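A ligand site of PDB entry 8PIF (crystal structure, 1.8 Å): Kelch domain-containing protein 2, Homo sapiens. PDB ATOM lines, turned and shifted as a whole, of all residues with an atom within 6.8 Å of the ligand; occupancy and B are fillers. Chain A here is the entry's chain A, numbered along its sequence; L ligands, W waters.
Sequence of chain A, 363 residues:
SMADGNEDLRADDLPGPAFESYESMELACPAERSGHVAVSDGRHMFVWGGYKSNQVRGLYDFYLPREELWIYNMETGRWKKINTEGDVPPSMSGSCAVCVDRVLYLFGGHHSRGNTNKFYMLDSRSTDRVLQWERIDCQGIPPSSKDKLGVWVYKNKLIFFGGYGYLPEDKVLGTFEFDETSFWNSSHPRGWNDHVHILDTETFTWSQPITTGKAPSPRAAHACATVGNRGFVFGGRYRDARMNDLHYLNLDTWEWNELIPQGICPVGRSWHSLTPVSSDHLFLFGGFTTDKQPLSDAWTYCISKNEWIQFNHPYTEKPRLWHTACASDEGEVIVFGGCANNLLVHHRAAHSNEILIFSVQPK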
ATOM      1  N   ASP A 147      12.679  10.572  -7.816  1.00  0.00           N
ATOM      2  CA  ASP A 147      13.704   9.627  -8.217  1.00  0.00           C
ATOM      3  C   ASP A 147      13.522   9.275  -9.710  1.00  0.00           C
ATOM      4  O   ASP A 147      12.586   9.774 -10.336  1.00  0.00           O
ATOM      5  CB  ASP A 147      13.626   8.374  -7.303  1.00  0.00           C
ATOM      6  CG  ASP A 147      12.370   7.513  -7.435  1.00  0.00           C
ATOM      7  OD1 ASP A 147      11.622   7.669  -8.439  1.00  0.00           O
ATOM      8  OD2 ASP A 147      12.118   6.695  -6.535  1.00  0.00           O
ATOM      9  N   LYS A 148      14.418   8.416 -10.276  1.00  0.00           N
ATOM     10  CA  LYS A 148      14.292   7.906 -11.644  1.00  0.00           C
ATOM     11  C   LYS A 148      14.109   9.058 -12.648  1.00  0.00           C
ATOM     12  O   LYS A 148      13.143   9.101 -13.412  1.00  0.00           O
ATOM     13  CB  LYS A 148      13.118   6.903 -11.731  1.00  0.00           C
ATOM     14  CG  LYS A 148      13.288   5.711 -10.775  1.00  0.00           C
ATOM     15  CD  LYS A 148      12.311   4.545 -11.055  1.00  0.00           C
ATOM     16  CE  LYS A 148      10.861   4.869 -10.763  1.00  0.00           C
ATOM     17  NZ  LYS A 148      10.611   5.191  -9.304  1.00  0.00           N
ATOM     18  N   GLY A 163      11.175  12.650 -13.735  1.00  0.00           N
ATOM     19  CA  GLY A 163      11.200  11.842 -12.532  1.00  0.00           C
ATOM     20  C   GLY A 163       9.856  11.503 -11.959  1.00  0.00           C
ATOM     21  O   GLY A 163       8.809  11.899 -12.494  1.00  0.00           O
ATOM     22  N   TYR A 164       9.875  10.771 -10.838  1.00  0.00           N
ATOM     23  CA  TYR A 164       8.672  10.289 -10.170  1.00  0.00           C
ATOM     24  C   TYR A 164       8.771  10.625  -8.687  1.00  0.00           C
ATOM     25  O   TYR A 164       9.765  10.316  -8.056  1.00  0.00           O
ATOM     26  CB  TYR A 164       8.573   8.762 -10.349  1.00  0.00           C
ATOM     27  CG  TYR A 164       7.279   8.158  -9.848  1.00  0.00           C
ATOM     28  CD1 TYR A 164       6.132   8.168 -10.633  1.00  0.00           C
ATOM     29  CD2 TYR A 164       7.204   7.541  -8.612  1.00  0.00           C
ATOM     30  CE1 TYR A 164       4.942   7.588 -10.182  1.00  0.00           C
ATOM     31  CE2 TYR A 164       6.035   6.958  -8.150  1.00  0.00           C
ATOM     32  CZ  TYR A 164       4.902   6.971  -8.935  1.00  0.00           C
ATOM     33  OH  TYR A 164       3.761   6.357  -8.472  1.00  0.00           O
ATOM     34  N   ASP A 179       0.009   9.558 -10.639  1.00  0.00           N
ATOM     35  CA  ASP A 179      -0.072   8.138 -10.961  1.00  0.00           C
ATOM     36  C   ASP A 179      -1.269   7.691 -10.113  1.00  0.00           C
ATOM     37  O   ASP A 179      -1.193   7.699  -8.872  1.00  0.00           O
ATOM     38  CB  ASP A 179       1.221   7.424 -10.555  1.00  0.00           C
ATOM     39  CG  ASP A 179       1.214   5.908 -10.693  1.00  0.00           C
ATOM     40  OD1 ASP A 179       0.211   5.364 -11.171  1.00  0.00           O
ATOM     41  OD2 ASP A 179       2.226   5.278 -10.323  1.00  0.00           O
ATOM     42  N   GLY A 191       3.560  11.044  -8.765  1.00  0.00           N
ATOM     43  CA  GLY A 191       3.355  11.122 -10.190  1.00  0.00           C
ATOM     44  C   GLY A 191       4.587  11.535 -10.956  1.00  0.00           C
ATOM     45  O   GLY A 191       5.661  11.728 -10.378  1.00  0.00           O
ATOM     46  N   TRP A 192       4.426  11.681 -12.273  1.00  0.00           N
ATOM     47  CA  TRP A 192       5.511  12.033 -13.209  1.00  0.00           C
ATOM     48  C   TRP A 192       5.540  13.526 -13.480  1.00  0.00           C
ATOM     49  O   TRP A 192       4.506  14.179 -13.421  1.00  0.00           O
ATOM     50  CB  TRP A 192       5.301  11.278 -14.542  1.00  0.00           C
ATOM     51  CG  TRP A 192       5.215   9.786 -14.371  1.00  0.00           C
ATOM     52  CD1 TRP A 192       6.265   8.919 -14.214  1.00  0.00           C
ATOM     53  CD2 TRP A 192       4.023   8.994 -14.265  1.00  0.00           C
ATOM     54  NE1 TRP A 192       5.803   7.637 -14.054  1.00  0.00           N
ATOM     55  CE2 TRP A 192       4.420   7.654 -14.112  1.00  0.00           C
ATOM     56  CE3 TRP A 192       2.652   9.294 -14.310  1.00  0.00           C
ATOM     57  CZ2 TRP A 192       3.498   6.604 -13.975  1.00  0.00           C
ATOM     58  CZ3 TRP A 192       1.728   8.256 -14.233  1.00  0.00           C
ATOM     59  CH2 TRP A 192       2.158   6.931 -14.041  1.00  0.00           C
ATOM     60  N   ARG A 219       7.627  12.076 -17.336  1.00  0.00           N
ATOM     61  CA  ARG A 219       8.125  10.699 -17.381  1.00  0.00           C
ATOM     62  C   ARG A 219       9.123  10.432 -16.311  1.00  0.00           C
ATOM     63  O   ARG A 219       9.715  11.370 -15.779  1.00  0.00           O
ATOM     64  CB  ARG A 219       8.777  10.381 -18.765  1.00  0.00           C
ATOM     65  CG  ARG A 219       9.953  11.313 -19.156  1.00  0.00           C
ATOM     66  CD  ARG A 219      10.338  11.116 -20.626  1.00  0.00           C
ATOM     67  NE  ARG A 219       9.240  11.491 -21.531  1.00  0.00           N
ATOM     68  CZ  ARG A 219       9.124  11.123 -22.803  1.00  0.00           C
ATOM     69  NH1 ARG A 219      10.046  10.354 -23.380  1.00  0.00           N
ATOM     70  NH2 ARG A 219       8.077  11.527 -23.518  1.00  0.00           N
ATOM     71  N   ALA A 220       9.378   9.156 -16.062  1.00  0.00           N
ATOM     72  CA  ALA A 220      10.416   8.713 -15.146  1.00  0.00           C
ATOM     73  C   ALA A 220      11.048   7.452 -15.744  1.00  0.00           C
ATOM     74  O   ALA A 220      10.454   6.813 -16.614  1.00  0.00           O
ATOM     75  CB  ALA A 220       9.811   8.427 -13.776  1.00  0.00           C
ATOM     76  N   ALA A 221      12.257   7.077 -15.288  1.00  0.00           N
ATOM     77  CA  ALA A 221      13.001   5.911 -15.797  1.00  0.00           C
ATOM     78  C   ALA A 221      13.350   6.067 -17.307  1.00  0.00           C
ATOM     79  O   ALA A 221      13.678   5.099 -18.007  1.00  0.00           O
ATOM     80  CB  ALA A 221      12.270   4.599 -15.479  1.00  0.00           C
ATOM     81  N   GLY A 236      11.287   6.159 -21.458  1.00  0.00           N
ATOM     82  CA  GLY A 236      10.773   6.393 -20.110  1.00  0.00           C
ATOM     83  C   GLY A 236       9.344   5.912 -19.945  1.00  0.00           C
ATOM     84  O   GLY A 236       8.663   5.549 -20.904  1.00  0.00           O
ATOM     85  N   ARG A 237       8.892   5.894 -18.699  1.00  0.00           N
ATOM     86  CA  ARG A 237       7.543   5.470 -18.345  1.00  0.00           C
ATOM     87  C   ARG A 237       6.652   6.707 -18.150  1.00  0.00           C
ATOM     88  O   ARG A 237       7.058   7.678 -17.511  1.00  0.00           O
ATOM     89  CB  ARG A 237       7.600   4.641 -17.060  1.00  0.00           C
ATOM     90  CG  ARG A 237       6.264   4.447 -16.301  1.00  0.00           C
ATOM     91  CD  ARG A 237       5.454   3.283 -16.790  1.00  0.00           C
ATOM     92  NE  ARG A 237       4.107   3.311 -16.217  1.00  0.00           N
ATOM     93  CZ  ARG A 237       3.764   2.940 -14.981  1.00  0.00           C
ATOM     94  NH1 ARG A 237       4.681   2.494 -14.126  1.00  0.00           N
ATOM     95  NH2 ARG A 237       2.506   3.037 -14.579  1.00  0.00           N
ATOM     96  N   TYR A 238       5.430   6.653 -18.684  1.00  0.00           N
ATOM     97  CA  TYR A 238       4.416   7.695 -18.496  1.00  0.00           C
ATOM     98  C   TYR A 238       3.066   7.032 -18.624  1.00  0.00           C
ATOM     99  O   TYR A 238       2.829   6.327 -19.598  1.00  0.00           O
ATOM    100  CB  TYR A 238       4.572   8.807 -19.535  1.00  0.00           C
ATOM    101  CG  TYR A 238       3.475   9.843 -19.527  1.00  0.00           C
ATOM    102  CD1 TYR A 238       3.168  10.562 -18.371  1.00  0.00           C
ATOM    103  CD2 TYR A 238       2.779  10.155 -20.685  1.00  0.00           C
ATOM    104  CE1 TYR A 238       2.215  11.559 -18.370  1.00  0.00           C
ATOM    105  CE2 TYR A 238       1.778  11.136 -20.685  1.00  0.00           C
ATOM    106  CZ  TYR A 238       1.516  11.848 -19.538  1.00  0.00           C
ATOM    107  OH  TYR A 238       0.535  12.804 -19.546  1.00  0.00           O
ATOM    108  N   ALA A 241       2.378   3.546 -20.568  1.00  0.00           N
ATOM    109  CA  ALA A 241       3.315   3.305 -21.650  1.00  0.00           C
ATOM    110  C   ALA A 241       4.785   3.465 -21.255  1.00  0.00           C
ATOM    111  O   ALA A 241       5.111   4.277 -20.393  1.00  0.00           O
ATOM    112  CB  ALA A 241       3.000   4.241 -22.810  1.00  0.00           C
ATOM    113  N   ARG A 242       5.656   2.671 -21.893  1.00  0.00           N
ATOM    114  CA  ARG A 242       7.112   2.762 -21.817  1.00  0.00           C
ATOM    115  C   ARG A 242       7.417   3.156 -23.254  1.00  0.00           C
ATOM    116  O   ARG A 242       7.185   2.388 -24.177  1.00  0.00           O
ATOM    117  CB  ARG A 242       7.747   1.447 -21.342  1.00  0.00           C
ATOM    118  CG  ARG A 242       7.280   1.152 -19.909  1.00  0.00           C
ATOM    119  CD  ARG A 242       8.087   0.137 -19.141  1.00  0.00           C
ATOM    120  NE  ARG A 242       7.557   0.030 -17.774  1.00  0.00           N
ATOM    121  CZ  ARG A 242       6.503  -0.706 -17.376  1.00  0.00           C
ATOM    122  NH1 ARG A 242       5.856  -1.491 -18.243  1.00  0.00           N
ATOM    123  NH2 ARG A 242       6.101  -0.685 -16.111  1.00  0.00           N
ATOM    124  N   ARG A 269      10.730   1.765 -24.235  1.00  0.00           N
ATOM    125  CA  ARG A 269      11.190   1.168 -22.992  1.00  0.00           C
ATOM    126  C   ARG A 269      11.452   2.235 -21.897  1.00  0.00           C
ATOM    127  O   ARG A 269      11.551   3.425 -22.159  1.00  0.00           O
ATOM    128  CB  ARG A 269      12.520   0.440 -23.295  1.00  0.00           C
ATOM    129  CG  ARG A 269      13.624   1.456 -23.779  1.00  0.00           C
ATOM    130  CD  ARG A 269      14.844   0.786 -24.346  1.00  0.00           C
ATOM    131  NE  ARG A 269      14.591   0.182 -25.653  1.00  0.00           N
ATOM    132  CZ  ARG A 269      15.381  -0.725 -26.228  1.00  0.00           C
ATOM    133  NH1 ARG A 269      16.502  -1.134 -25.632  1.00  0.00           N
ATOM    134  NH2 ARG A 269      15.045  -1.233 -27.409  1.00  0.00           N
ATOM    135  N   SER A 270      11.626   1.750 -20.661  1.00  0.00           N
ATOM    136  CA  SER A 270      12.100   2.525 -19.536  1.00  0.00           C
ATOM    137  C   SER A 270      13.219   1.693 -18.899  1.00  0.00           C
ATOM    138  O   SER A 270      13.390   0.512 -19.264  1.00  0.00           O
ATOM    139  CB  SER A 270      10.967   2.779 -18.527  1.00  0.00           C
ATOM    140  OG  SER A 270      10.701   1.616 -17.758  1.00  0.00           O
ATOM    141  N   TRP A 271      13.956   2.261 -17.915  1.00  0.00           N
ATOM    142  CA  TRP A 271      14.984   1.530 -17.181  1.00  0.00           C
ATOM    143  C   TRP A 271      16.155   1.022 -18.053  1.00  0.00           C
ATOM    144  O   TRP A 271      16.922   0.161 -17.639  1.00  0.00           O
ATOM    145  CB  TRP A 271      14.354   0.389 -16.337  1.00  0.00           C
ATOM    146  CG  TRP A 271      13.802   0.831 -15.016  1.00  0.00           C
ATOM    147  CD1 TRP A 271      14.354   1.742 -14.154  1.00  0.00           C
ATOM    148  CD2 TRP A 271      12.745   0.176 -14.291  1.00  0.00           C
ATOM    149  NE1 TRP A 271      13.618   1.786 -12.984  1.00  0.00           N
ATOM    150  CE2 TRP A 271      12.647   0.814 -13.029  1.00  0.00           C
ATOM    151  CE3 TRP A 271      11.825  -0.823 -14.615  1.00  0.00           C
ATOM    152  CZ2 TRP A 271      11.667   0.475 -12.101  1.00  0.00           C
ATOM    153  CZ3 TRP A 271      10.834  -1.143 -13.698  1.00  0.00           C
ATOM    154  CH2 TRP A 271      10.772  -0.506 -12.456  1.00  0.00           C
ATOM    155  N   PHE A 288      13.008  -2.136 -20.326  1.00  0.00           N
ATOM    156  CA  PHE A 288      11.793  -2.884 -20.061  1.00  0.00           C
ATOM    157  C   PHE A 288      10.670  -2.297 -20.931  1.00  0.00           C
ATOM    158  O   PHE A 288      10.454  -1.091 -20.888  1.00  0.00           O
ATOM    159  CB  PHE A 288      11.535  -2.678 -18.549  1.00  0.00           C
ATOM    160  CG  PHE A 288      10.495  -3.540 -17.878  1.00  0.00           C
ATOM    161  CD1 PHE A 288      10.635  -4.923 -17.848  1.00  0.00           C
ATOM    162  CD2 PHE A 288       9.500  -2.973 -17.106  1.00  0.00           C
ATOM    163  CE1 PHE A 288       9.732  -5.708 -17.157  1.00  0.00           C
ATOM    164  CE2 PHE A 288       8.605  -3.764 -16.405  1.00  0.00           C
ATOM    165  CZ  PHE A 288       8.719  -5.118 -16.446  1.00  0.00           C
ATOM    166  N   LEU A 344       9.634  -5.834 -10.662  1.00  0.00           N
ATOM    167  CA  LEU A 344       8.398  -5.515  -9.946  1.00  0.00           C
ATOM    168  C   LEU A 344       7.831  -6.762  -9.218  1.00  0.00           C
ATOM    169  O   LEU A 344       7.094  -6.589  -8.252  1.00  0.00           O
ATOM    170  CB  LEU A 344       7.346  -4.881 -10.887  1.00  0.00           C
ATOM    171  CG  LEU A 344       7.797  -3.590 -11.638  1.00  0.00           C
ATOM    172  CD1 LEU A 344       6.815  -3.250 -12.750  1.00  0.00           C
ATOM    173  CD2 LEU A 344       7.974  -2.406 -10.658  1.00  0.00           C
HETATM  174  C1  LIG L   1       9.067   2.711 -13.687  1.00  0.00           C
HETATM  175  C2  LIG L   1       6.640   5.007 -12.160  1.00  0.00           C
HETATM  176  C3  LIG L   1       8.350   1.885 -14.744  1.00  0.00           C
HETATM  177  C4  LIG L   1       8.245   3.869 -13.189  1.00  0.00           C
HETATM  178  C5  LIG L   1       7.181   3.795 -12.240  1.00  0.00           C
HETATM  179  C6  LIG L   1       8.259   5.140 -13.604  1.00  0.00           C
HETATM  180  O1  LIG L   1       7.294   5.865 -13.006  1.00  0.00           O
HETATM  181  O2  LIG L   1       8.860   1.815 -15.886  1.00  0.00           O
HETATM  182  O3  LIG L   1       7.269   1.337 -14.402  1.00  0.00           O
HETATM  183  O   HOH W   1       7.816   4.249  -9.383  1.00  0.00           O
HETATM  184  O   HOH W   2       6.654   0.630 -11.889  1.00  0.00           O
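The backbone carbonyl oxygen of Ser 270 sits at hydrogen-bond distance from the backbone NH of Phe 288 (2.9 Å). The backbone NH (N) of Arg 237 is in hydrogen-bond range of the backbone carbonyl oxygen (O) of Ala 220, 2.8 Å away. OH of Tyr 164 sits at hydrogen-bond distance from OD2 of Asp 179 (2.6 Å). N of Tyr 164 sits at hydrogen-bond distance from O of Asp 147, 2.9 Å away. O of Lys 148 lies within hydrogen-bond range of N of Ala 221, at 2.9 Å. The side-chain amino group of Lys 148 is in salt-bridge range of the side-chain carboxylate of Asp 147. O of Ala 221 is in hydrogen-bond range of N of Trp 271.
CE of Lys 148 touches C4 of the ligand, 3.7 Å away. CD1 of Tyr 164 touches O1 of the ligand, 3.5 Å away. CB of Ala 220 touches C6 of the ligand (3.6 Å). Trp 271 touches the ligand (CZ2 to C1, 3.8 Å). Hydrophobic or aromatic side chains within 4 Å of the ligand: Tyr 164, Trp 192, Ala 220 and Trp 271. Of the 20 residues printed, 8 come within 4 Å of the ligand. Along chain A the residues within 4 Å of the ligand span positions 148 to 271.
The indole nitrogen (NE1) of Trp 192 sits at hydrogen-bond distance from an oxygen (O1) of the ligand, at 2.5 Å. O2 of the ligand is in hydrogen-bond range of OG of Ser 270. NH1 of Arg 237 lies within salt-bridge range of O3 of the ligand, 2.8 Å away. An oxygen (O3) of the ligand lies within salt-bridge range of the guanidinium group of Arg 242 (2.9 Å).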
